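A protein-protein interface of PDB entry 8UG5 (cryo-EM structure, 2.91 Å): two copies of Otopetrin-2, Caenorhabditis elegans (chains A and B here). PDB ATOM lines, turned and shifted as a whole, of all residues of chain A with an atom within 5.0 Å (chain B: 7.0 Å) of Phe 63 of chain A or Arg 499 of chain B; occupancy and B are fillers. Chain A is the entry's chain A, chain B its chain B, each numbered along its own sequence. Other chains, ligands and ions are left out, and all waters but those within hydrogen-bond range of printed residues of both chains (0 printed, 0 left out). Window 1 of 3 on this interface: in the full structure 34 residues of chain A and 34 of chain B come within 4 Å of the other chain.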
ATOM      1  N   ARG A  59     -16.167  34.250  15.919  1.00  0.00           N
ATOM      2  CA  ARG A  59     -15.621  33.431  14.809  1.00  0.00           C
ATOM      3  C   ARG A  59     -16.612  32.340  14.428  1.00  0.00           C
ATOM      4  O   ARG A  59     -16.411  31.706  13.386  1.00  0.00           O
ATOM      5  CB  ARG A  59     -14.249  32.885  15.196  1.00  0.00           C
ATOM      6  CG  ARG A  59     -13.177  33.956  15.339  1.00  0.00           C
ATOM      7  CD  ARG A  59     -11.809  33.392  15.678  1.00  0.00           C
ATOM      8  NE  ARG A  59     -10.816  34.438  15.878  1.00  0.00           N
ATOM      9  CZ  ARG A  59      -9.574  34.223  16.294  1.00  0.00           C
ATOM     10  NH1 ARG A  59      -9.009  35.058  17.148  1.00  0.00           N
ATOM     11  NH2 ARG A  59      -8.898  33.176  15.852  1.00  0.00           N
ATOM     12  N   ALA A  60     -17.649  32.161  15.224  1.00  0.00           N
ATOM     13  CA  ALA A  60     -18.701  31.197  14.880  1.00  0.00           C
ATOM     14  C   ALA A  60     -19.692  31.949  14.021  1.00  0.00           C
ATOM     15  O   ALA A  60     -20.144  31.391  13.011  1.00  0.00           O
ATOM     16  CB  ALA A  60     -19.326  30.698  16.131  1.00  0.00           C
ATOM     17  N   THR A  61     -19.978  33.189  14.410  1.00  0.00           N
ATOM     18  CA  THR A  61     -20.898  34.011  13.630  1.00  0.00           C
ATOM     19  C   THR A  61     -20.266  34.450  12.318  1.00  0.00           C
ATOM     20  O   THR A  61     -20.954  34.564  11.297  1.00  0.00           O
ATOM     21  CB  THR A  61     -21.341  35.227  14.440  1.00  0.00           C
ATOM     22  OG1 THR A  61     -20.190  35.862  15.013  1.00  0.00           O
ATOM     23  CG2 THR A  61     -22.287  34.808  15.544  1.00  0.00           C
ATOM     24  N   ASN A  62     -18.942  34.627  12.339  1.00  0.00           N
ATOM     25  CA  ASN A  62     -18.216  34.975  11.091  1.00  0.00           C
ATOM     26  C   ASN A  62     -18.468  33.874  10.057  1.00  0.00           C
ATOM     27  O   ASN A  62     -19.062  34.177   9.004  1.00  0.00           O
ATOM     28  CB  ASN A  62     -16.719  35.162  11.337  1.00  0.00           C
ATOM     29  CG  ASN A  62     -16.164  36.395  10.657  1.00  0.00           C
ATOM     30  OD1 ASN A  62     -16.541  36.709   9.531  1.00  0.00           O
ATOM     31  ND2 ASN A  62     -15.273  37.100  11.335  1.00  0.00           N
ATOM     32  N   PHE A  63     -18.028  32.645  10.351  1.00  0.00           N
ATOM     33  CA  PHE A  63     -18.212  31.545   9.389  1.00  0.00           C
ATOM     34  C   PHE A  63     -19.689  31.438   9.043  1.00  0.00           C
ATOM     35  O   PHE A  63     -19.989  31.305   7.867  1.00  0.00           O
ATOM     36  CB  PHE A  63     -17.571  30.234   9.865  1.00  0.00           C
ATOM     37  CG  PHE A  63     -18.195  28.955   9.374  1.00  0.00           C
ATOM     38  CD1 PHE A  63     -17.813  28.392   8.170  1.00  0.00           C
ATOM     39  CD2 PHE A  63     -19.155  28.305  10.128  1.00  0.00           C
ATOM     40  CE1 PHE A  63     -18.394  27.220   7.721  1.00  0.00           C
ATOM     41  CE2 PHE A  63     -19.738  27.135   9.676  1.00  0.00           C
ATOM     42  CZ  PHE A  63     -19.355  26.596   8.474  1.00  0.00           C
ATOM     43  N   PHE A  64     -20.587  31.477  10.023  1.00  0.00           N
ATOM     44  CA  PHE A  64     -21.968  31.263   9.604  1.00  0.00           C
ATOM     45  C   PHE A  64     -22.378  32.257   8.527  1.00  0.00           C
ATOM     46  O   PHE A  64     -23.010  31.879   7.535  1.00  0.00           O
ATOM     47  CB  PHE A  64     -22.915  31.357  10.798  1.00  0.00           C
ATOM     48  CG  PHE A  64     -24.335  30.989  10.469  1.00  0.00           C
ATOM     49  CD1 PHE A  64     -24.651  29.713  10.047  1.00  0.00           C
ATOM     50  CD2 PHE A  64     -25.349  31.922  10.564  1.00  0.00           C
ATOM     51  CE1 PHE A  64     -25.949  29.366   9.733  1.00  0.00           C
ATOM     52  CE2 PHE A  64     -26.648  31.583  10.253  1.00  0.00           C
ATOM     53  CZ  PHE A  64     -26.949  30.302   9.836  1.00  0.00           C
ATOM     54  N   VAL A  65     -22.027  33.531   8.705  1.00  0.00           N
ATOM     55  CA  VAL A  65     -22.363  34.540   7.705  1.00  0.00           C
ATOM     56  C   VAL A  65     -21.607  34.274   6.409  1.00  0.00           C
ATOM     57  O   VAL A  65     -22.165  34.398   5.312  1.00  0.00           O
ATOM     58  CB  VAL A  65     -22.081  35.950   8.253  1.00  0.00           C
ATOM     59  CG1 VAL A  65     -22.205  36.982   7.150  1.00  0.00           C
ATOM     60  CG2 VAL A  65     -23.029  36.270   9.392  1.00  0.00           C
ATOM     61  N   ARG A  66     -20.330  33.897   6.516  1.00  0.00           N
ATOM     62  CA  ARG A  66     -19.557  33.547   5.328  1.00  0.00           C
ATOM     63  C   ARG A  66     -20.213  32.403   4.568  1.00  0.00           C
ATOM     64  O   ARG A  66     -20.364  32.462   3.344  1.00  0.00           O
ATOM     65  CB  ARG A  66     -18.131  33.166   5.722  1.00  0.00           C
ATOM     66  CG  ARG A  66     -17.125  34.291   5.654  1.00  0.00           C
ATOM     67  CD  ARG A  66     -15.718  33.732   5.725  1.00  0.00           C
ATOM     68  NE  ARG A  66     -14.706  34.773   5.619  1.00  0.00           N
ATOM     69  CZ  ARG A  66     -13.401  34.543   5.584  1.00  0.00           C
ATOM     70  NH1 ARG A  66     -12.915  33.315   5.633  1.00  0.00           N
ATOM     71  NH2 ARG A  66     -12.563  35.572   5.497  1.00  0.00           N
ATOM     72  N   LEU A  67     -20.620  31.355   5.284  1.00  0.00           N
ATOM     73  CA  LEU A  67     -21.242  30.202   4.644  1.00  0.00           C
ATOM     74  C   LEU A  67     -22.574  30.569   4.007  1.00  0.00           C
ATOM     75  O   LEU A  67     -22.862  30.148   2.883  1.00  0.00           O
ATOM     76  CB  LEU A  67     -21.430  29.079   5.661  1.00  0.00           C
ATOM     77  CG  LEU A  67     -22.463  28.004   5.318  1.00  0.00           C
ATOM     78  CD1 LEU A  67     -21.978  27.134   4.173  1.00  0.00           C
ATOM     79  CD2 LEU A  67     -22.775  27.160   6.533  1.00  0.00           C
ATOM     80  N   ILE A  68     -23.399  31.350   4.708  1.00  0.00           N
ATOM     81  CA  ILE A  68     -24.699  31.730   4.162  1.00  0.00           C
ATOM     82  C   ILE A  68     -24.535  32.578   2.909  1.00  0.00           C
ATOM     83  O   ILE A  68     -25.205  32.347   1.895  1.00  0.00           O
ATOM     84  CB  ILE A  68     -25.537  32.453   5.231  1.00  0.00           C
ATOM     85  CG1 ILE A  68     -25.960  31.478   6.327  1.00  0.00           C
ATOM     86  CG2 ILE A  68     -26.759  33.086   4.605  1.00  0.00           C
ATOM     87  CD1 ILE A  68     -26.906  30.407   5.849  1.00  0.00           C
ATOM     88  N   GLN B 428     -21.482  25.104  21.325  1.00  0.00           N
ATOM     89  CA  GLN B 428     -20.274  25.910  21.280  1.00  0.00           C
ATOM     90  C   GLN B 428     -19.487  25.613  20.013  1.00  0.00           C
ATOM     91  O   GLN B 428     -19.491  24.487  19.507  1.00  0.00           O
ATOM     92  CB  GLN B 428     -19.388  25.663  22.512  1.00  0.00           C
ATOM     93  CG  GLN B 428     -20.028  26.025  23.851  1.00  0.00           C
ATOM     94  CD  GLN B 428     -21.137  25.075  24.255  1.00  0.00           C
ATOM     95  OE1 GLN B 428     -21.296  24.007  23.668  1.00  0.00           O
ATOM     96  NE2 GLN B 428     -21.915  25.465  25.255  1.00  0.00           N
ATOM     97  N   TYR B 429     -18.800  26.653  19.530  1.00  0.00           N
ATOM     98  CA  TYR B 429     -17.935  26.493  18.338  1.00  0.00           C
ATOM     99  C   TYR B 429     -16.756  25.600  18.713  1.00  0.00           C
ATOM    100  O   TYR B 429     -16.262  25.694  19.852  1.00  0.00           O
ATOM    101  CB  TYR B 429     -17.417  27.857  17.882  1.00  0.00           C
ATOM    102  CG  TYR B 429     -17.034  27.943  16.428  1.00  0.00           C
ATOM    103  CD1 TYR B 429     -17.723  27.224  15.464  1.00  0.00           C
ATOM    104  CD2 TYR B 429     -15.994  28.757  16.011  1.00  0.00           C
ATOM    105  CE1 TYR B 429     -17.385  27.310  14.125  1.00  0.00           C
ATOM    106  CE2 TYR B 429     -15.644  28.855  14.676  1.00  0.00           C
ATOM    107  CZ  TYR B 429     -16.343  28.128  13.729  1.00  0.00           C
ATOM    108  OH  TYR B 429     -15.998  28.212  12.403  1.00  0.00           O
ATOM    109  N   ARG B 430     -16.312  24.775  17.771  1.00  0.00           N
ATOM    110  CA  ARG B 430     -15.181  23.850  18.021  1.00  0.00           C
ATOM    111  C   ARG B 430     -13.870  24.628  18.137  1.00  0.00           C
ATOM    112  O   ARG B 430     -13.767  25.725  17.551  1.00  0.00           O
ATOM    113  CB  ARG B 430     -15.105  22.799  16.906  1.00  0.00           C
ATOM    114  CG  ARG B 430     -14.240  23.180  15.714  1.00  0.00           C
ATOM    115  CD  ARG B 430     -14.846  24.290  14.884  1.00  0.00           C
ATOM    116  NE  ARG B 430     -13.930  24.772  13.862  1.00  0.00           N
ATOM    117  CZ  ARG B 430     -13.443  26.005  13.811  1.00  0.00           C
ATOM    118  NH1 ARG B 430     -13.662  26.840  14.810  1.00  0.00           N
ATOM    119  NH2 ARG B 430     -12.749  26.400  12.760  1.00  0.00           N
ATOM    120  N   LEU B 431     -12.945  24.100  18.893  1.00  0.00           N
ATOM    121  CA  LEU B 431     -11.624  24.702  19.009  1.00  0.00           C
ATOM    122  C   LEU B 431     -10.624  24.106  18.028  1.00  0.00           C
ATOM    123  O   LEU B 431      -9.724  24.818  17.568  1.00  0.00           O
ATOM    124  CB  LEU B 431     -11.094  24.563  20.441  1.00  0.00           C
ATOM    125  CG  LEU B 431     -10.628  23.196  20.953  1.00  0.00           C
ATOM    126  CD1 LEU B 431      -9.811  23.366  22.223  1.00  0.00           C
ATOM    127  CD2 LEU B 431     -11.801  22.262  21.206  1.00  0.00           C
ATOM    128  N   ALA B 433     -10.501  22.107  14.367  1.00  0.00           N
ATOM    129  CA  ALA B 433     -11.184  21.589  13.190  1.00  0.00           C
ATOM    130  C   ALA B 433     -10.699  20.171  12.924  1.00  0.00           C
ATOM    131  O   ALA B 433      -9.492  19.909  12.951  1.00  0.00           O
ATOM    132  CB  ALA B 433     -10.927  22.488  11.982  1.00  0.00           C
ATOM    133  N   GLU B 436     -12.817  18.962   8.405  1.00  0.00           N
ATOM    134  CA  GLU B 436     -13.833  19.910   7.966  1.00  0.00           C
ATOM    135  C   GLU B 436     -13.639  20.365   6.529  1.00  0.00           C
ATOM    136  O   GLU B 436     -14.562  20.939   5.945  1.00  0.00           O
ATOM    137  CB  GLU B 436     -13.852  21.129   8.888  1.00  0.00           C
ATOM    138  CG  GLU B 436     -14.303  20.831  10.299  1.00  0.00           C
ATOM    139  CD  GLU B 436     -14.330  22.071  11.157  1.00  0.00           C
ATOM    140  OE1 GLU B 436     -13.928  23.141  10.654  1.00  0.00           O
ATOM    141  OE2 GLU B 436     -14.746  21.977  12.329  1.00  0.00           O
ATOM    142  N   VAL B 437     -12.478  20.114   5.938  1.00  0.00           N
ATOM    143  CA  VAL B 437     -12.160  20.571   4.593  1.00  0.00           C
ATOM    144  C   VAL B 437     -12.603  19.556   3.548  1.00  0.00           C
ATOM    145  O   VAL B 437     -13.192  19.918   2.531  1.00  0.00           O
ATOM    146  CB  VAL B 437     -10.657  20.887   4.453  1.00  0.00           C
ATOM    147  CG1 VAL B 437     -10.367  21.454   3.077  1.00  0.00           C
ATOM    148  CG2 VAL B 437     -10.213  21.855   5.538  1.00  0.00           C
ATOM    149  N   GLU B 440     -16.264  19.727   3.560  1.00  0.00           N
ATOM    150  CA  GLU B 440     -16.683  20.911   2.823  1.00  0.00           C
ATOM    151  C   GLU B 440     -16.618  20.674   1.321  1.00  0.00           C
ATOM    152  O   GLU B 440     -17.570  20.969   0.596  1.00  0.00           O
ATOM    153  CB  GLU B 440     -15.808  22.100   3.216  1.00  0.00           C
ATOM    154  CG  GLU B 440     -16.415  22.987   4.280  1.00  0.00           C
ATOM    155  CD  GLU B 440     -15.408  23.939   4.885  1.00  0.00           C
ATOM    156  OE1 GLU B 440     -14.213  23.590   4.935  1.00  0.00           O
ATOM    157  OE2 GLU B 440     -15.815  25.040   5.305  1.00  0.00           O
ATOM    158  N   ALA B 492     -26.154  23.950   4.775  1.00  0.00           N
ATOM    159  CA  ALA B 492     -25.810  24.896   5.831  1.00  0.00           C
ATOM    160  C   ALA B 492     -25.839  24.226   7.201  1.00  0.00           C
ATOM    161  O   ALA B 492     -24.933  24.423   8.018  1.00  0.00           O
ATOM    162  CB  ALA B 492     -26.758  26.091   5.796  1.00  0.00           C
ATOM    163  N   PHE B 493     -26.922  23.476   7.448  1.00  0.00           N
ATOM    164  CA  PHE B 493     -27.097  22.780   8.749  1.00  0.00           C
ATOM    165  C   PHE B 493     -25.876  21.902   8.999  1.00  0.00           C
ATOM    166  O   PHE B 493     -25.288  22.002  10.072  1.00  0.00           O
ATOM    167  CB  PHE B 493     -28.365  21.922   8.742  1.00  0.00           C
ATOM    168  CG  PHE B 493     -28.576  21.095   9.985  1.00  0.00           C
ATOM    169  CD1 PHE B 493     -29.192  21.643  11.098  1.00  0.00           C
ATOM    170  CD2 PHE B 493     -28.161  19.775  10.048  1.00  0.00           C
ATOM    171  CE1 PHE B 493     -29.385  20.890  12.245  1.00  0.00           C
ATOM    172  CE2 PHE B 493     -28.343  19.028  11.200  1.00  0.00           C
ATOM    173  CZ  PHE B 493     -28.965  19.583  12.293  1.00  0.00           C
ATOM    174  N   ILE B 494     -25.530  21.050   8.037  1.00  0.00           N
ATOM    175  CA  ILE B 494     -24.399  20.114   8.284  1.00  0.00           C
ATOM    176  C   ILE B 494     -23.132  20.942   8.494  1.00  0.00           C
ATOM    177  O   ILE B 494     -22.589  20.873   9.599  1.00  0.00           O
ATOM    178  CB  ILE B 494     -24.264  19.081   7.150  1.00  0.00           C
ATOM    179  CG1 ILE B 494     -25.426  18.088   7.170  1.00  0.00           C
ATOM    180  CG2 ILE B 494     -22.926  18.367   7.227  1.00  0.00           C
ATOM    181  CD1 ILE B 494     -25.553  17.285   5.906  1.00  0.00           C
ATOM    182  N   LEU B 495     -22.732  21.749   7.509  1.00  0.00           N
ATOM    183  CA  LEU B 495     -21.452  22.504   7.606  1.00  0.00           C
ATOM    184  C   LEU B 495     -21.375  23.307   8.910  1.00  0.00           C
ATOM    185  O   LEU B 495     -20.242  23.549   9.367  1.00  0.00           O
ATOM    186  CB  LEU B 495     -21.295  23.403   6.378  1.00  0.00           C
ATOM    187  CG  LEU B 495     -20.736  22.699   5.143  1.00  0.00           C
ATOM    188  CD1 LEU B 495     -20.180  23.701   4.144  1.00  0.00           C
ATOM    189  CD2 LEU B 495     -19.674  21.684   5.538  1.00  0.00           C
ATOM    190  N   THR B 496     -22.515  23.690   9.497  1.00  0.00           N
ATOM    191  CA  THR B 496     -22.451  24.400  10.769  1.00  0.00           C
ATOM    192  C   THR B 496     -22.344  23.437  11.944  1.00  0.00           C
ATOM    193  O   THR B 496     -21.437  23.562  12.773  1.00  0.00           O
ATOM    194  CB  THR B 496     -23.676  25.295  10.935  1.00  0.00           C
ATOM    195  OG1 THR B 496     -24.856  24.551  10.611  1.00  0.00           O
ATOM    196  CG2 THR B 496     -23.576  26.485  10.022  1.00  0.00           C
ATOM    197  N   THR B 497     -23.262  22.474  12.034  1.00  0.00           N
ATOM    198  CA  THR B 497     -23.284  21.567  13.172  1.00  0.00           C
ATOM    199  C   THR B 497     -22.064  20.658  13.220  1.00  0.00           C
ATOM    200  O   THR B 497     -21.762  20.108  14.283  1.00  0.00           O
ATOM    201  CB  THR B 497     -24.561  20.731  13.149  1.00  0.00           C
ATOM    202  OG1 THR B 497     -24.626  19.994  11.926  1.00  0.00           O
ATOM    203  CG2 THR B 497     -25.776  21.632  13.246  1.00  0.00           C
ATOM    204  N   SER B 498     -21.318  20.553  12.107  1.00  0.00           N
ATOM    205  CA  SER B 498     -20.054  19.762  12.085  1.00  0.00           C
ATOM    206  C   SER B 498     -18.978  20.510  12.869  1.00  0.00           C
ATOM    207  O   SER B 498     -17.935  19.900  13.140  1.00  0.00           O
ATOM    208  CB  SER B 498     -19.590  19.494  10.679  1.00  0.00           C
ATOM    209  OG  SER B 498     -20.691  19.212   9.830  1.00  0.00           O
ATOM    210  N   ARG B 499     -19.176  21.803  13.122  1.00  0.00           N
ATOM    211  CA  ARG B 499     -18.285  22.603  13.946  1.00  0.00           C
ATOM    212  C   ARG B 499     -18.850  22.887  15.329  1.00  0.00           C
ATOM    213  O   ARG B 499     -18.250  23.657  16.082  1.00  0.00           O
ATOM    214  CB  ARG B 499     -17.965  23.920  13.239  1.00  0.00           C
ATOM    215  CG  ARG B 499     -17.472  23.741  11.818  1.00  0.00           C
ATOM    216  CD  ARG B 499     -16.650  24.931  11.371  1.00  0.00           C
ATOM    217  NE  ARG B 499     -16.467  24.947   9.926  1.00  0.00           N
ATOM    218  CZ  ARG B 499     -15.538  25.653   9.298  1.00  0.00           C
ATOM    219  NH1 ARG B 499     -14.687  26.420   9.960  1.00  0.00           N
ATOM    220  NH2 ARG B 499     -15.459  25.584   7.973  1.00  0.00           N
ATOM    221  N   LEU B 500     -19.982  22.286  15.679  1.00  0.00           N
ATOM    222  CA  LEU B 500     -20.635  22.526  16.957  1.00  0.00           C
ATOM    223  C   LEU B 500     -20.462  21.313  17.859  1.00  0.00           C
ATOM    224  O   LEU B 500     -20.711  20.180  17.437  1.00  0.00           O
ATOM    225  CB  LEU B 500     -22.116  22.830  16.756  1.00  0.00           C
ATOM    226  CG  LEU B 500     -22.402  24.237  16.248  1.00  0.00           C
ATOM    227  CD1 LEU B 500     -23.896  24.496  16.218  1.00  0.00           C
ATOM    228  CD2 LEU B 500     -21.692  25.247  17.120  1.00  0.00           C
ATOM    229  N   ARG B 501     -20.037  21.553  19.094  1.00  0.00           N
ATOM    230  CA  ARG B 501     -19.811  20.492  20.059  1.00  0.00           C
ATOM    231  C   ARG B 501     -20.495  20.836  21.371  1.00  0.00           C
ATOM    232  O   ARG B 501     -20.603  22.004  21.749  1.00  0.00           O
ATOM    233  CB  ARG B 501     -18.315  20.262  20.300  1.00  0.00           C
ATOM    234  CG  ARG B 501     -17.656  19.376  19.261  1.00  0.00           C
ATOM    235  CD  ARG B 501     -17.193  20.199  18.079  1.00  0.00           C
ATOM    236  NE  ARG B 501     -16.126  19.549  17.331  1.00  0.00           N
ATOM    237  CZ  ARG B 501     -16.302  18.908  16.185  1.00  0.00           C
ATOM    238  NH1 ARG B 501     -17.467  18.920  15.560  1.00  0.00           N
ATOM    239  NH2 ARG B 501     -15.283  18.243  15.651  1.00  0.00           N
ATOM    240  N   ILE B 575     -21.473  13.713  12.854  1.00  0.00           N
ATOM    241  CA  ILE B 575     -22.011  14.731  13.753  1.00  0.00           C
ATOM    242  C   ILE B 575     -22.669  14.079  14.959  1.00  0.00           C
ATOM    243  O   ILE B 575     -22.481  14.516  16.101  1.00  0.00           O
ATOM    244  CB  ILE B 575     -22.990  15.647  12.998  1.00  0.00           C
ATOM    245  CG1 ILE B 575     -22.242  16.496  11.971  1.00  0.00           C
ATOM    246  CG2 ILE B 575     -23.736  16.544  13.965  1.00  0.00           C
ATOM    247  CD1 ILE B 575     -23.148  17.296  11.081  1.00  0.00           C
ATOM    248  N   THR B 579     -20.240  15.544  17.973  1.00  0.00           N
ATOM    249  CA  THR B 579     -20.888  16.599  18.748  1.00  0.00           C
ATOM    250  C   THR B 579     -21.307  16.097  20.125  1.00  0.00           C
ATOM    251  O   THR B 579     -21.116  16.787  21.133  1.00  0.00           O
ATOM    252  CB  THR B 579     -22.097  17.145  17.985  1.00  0.00           C
ATOM    253  OG1 THR B 579     -21.658  17.780  16.778  1.00  0.00           O
ATOM    254  CG2 THR B 579     -22.858  18.152  18.832  1.00  0.00           C
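The side-chain carboxylate (OE1) of Glu 436 of chain B lies within salt-bridge range of the guanidinium group (NE) of Arg 499 of chain B, at 3.2 Å. OG1 of Thr 496 of chain B lies within hydrogen-bond range of O of Phe 493 of chain B, at 2.6 Å. OG1 of Thr 496 of chain B sits at hydrogen-bond distance from O of Ala 492 of chain B (2.6 Å). O of Arg 499 of chain B is in hydrogen-bond range of N of Arg 430 of chain B (2.8 Å). The side-chain hydroxyl (OH) of Tyr 429 of chain B is in hydrogen-bond range of the guanidinium group (NH1) of Arg 499 of chain B (3.3 Å). The side-chain carboxylate of Glu 440 of chain B is in salt-bridge range of the guanidinium group of Arg 499 of chain B (2.7 Å).
Among the printed residues, merely in contact across the chains: Arg 59 of chain A with Tyr 429 of chain B (3.2 Å), Ala 60 of chain A with Tyr 429 of chain B (3.6 Å), Phe 63 of chain A with Tyr 429 of chain B (3.6 Å), Phe 63 of chain A with Leu 495 of chain B (3.3 Å), Phe 63 of chain A with Thr 496 of chain B (3.9 Å), Phe 63 of chain A with Arg 499 of chain B (3.4 Å), Phe 64 of chain A with Thr 496 of chain B (3.4 Å), Leu 67 of chain A with Ala 492 of chain B (3.8 Å), Leu 67 of chain A with Leu 495 of chain B (3.9 Å) and Leu 67 of chain A with Thr 496 of chain B (3.6 Å).
Of chain A, only Phe 63 (3.4 Å) comes within 4 Å of Arg 499 of chain B. Printed residues of chain A within 4 Å of Tyr 429 of chain B: Arg 59 (3.2 Å), Ala 60 (3.6 Å) and Phe 63 (3.6 Å). Printed residues of chain A within 4 Å of Ala 492 of chain B: Leu 67. Printed residues of chain B within 4 Å of Arg 59 of chain A: Tyr 429. Of the printed residues of chain A, Thr 496 of chain B touches Phe 63, Phe 64 and Leu 67. Asn 62 of chain A touches none of the printed residues of chain B. Leu 431 of chain B touches none of the printed residues of chain A. The nearest printed residue of chain A that does not touch Ala 492 of chain B is Ile 68 of chain A (4.3 Å).
Hydrophobic or aromatic side chains of chain A that line the printed part of chain B: Ala 60, Phe 63, Phe 64 and Leu 67. Of the 20 printed residues of chain B, 5 touch a printed residue of chain A. Among the printed residues, no Asp or Glu carboxylate lies within 4 Å of a Lys or Arg side-chain nitrogen of the other chain.
No position is printed for both chains.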
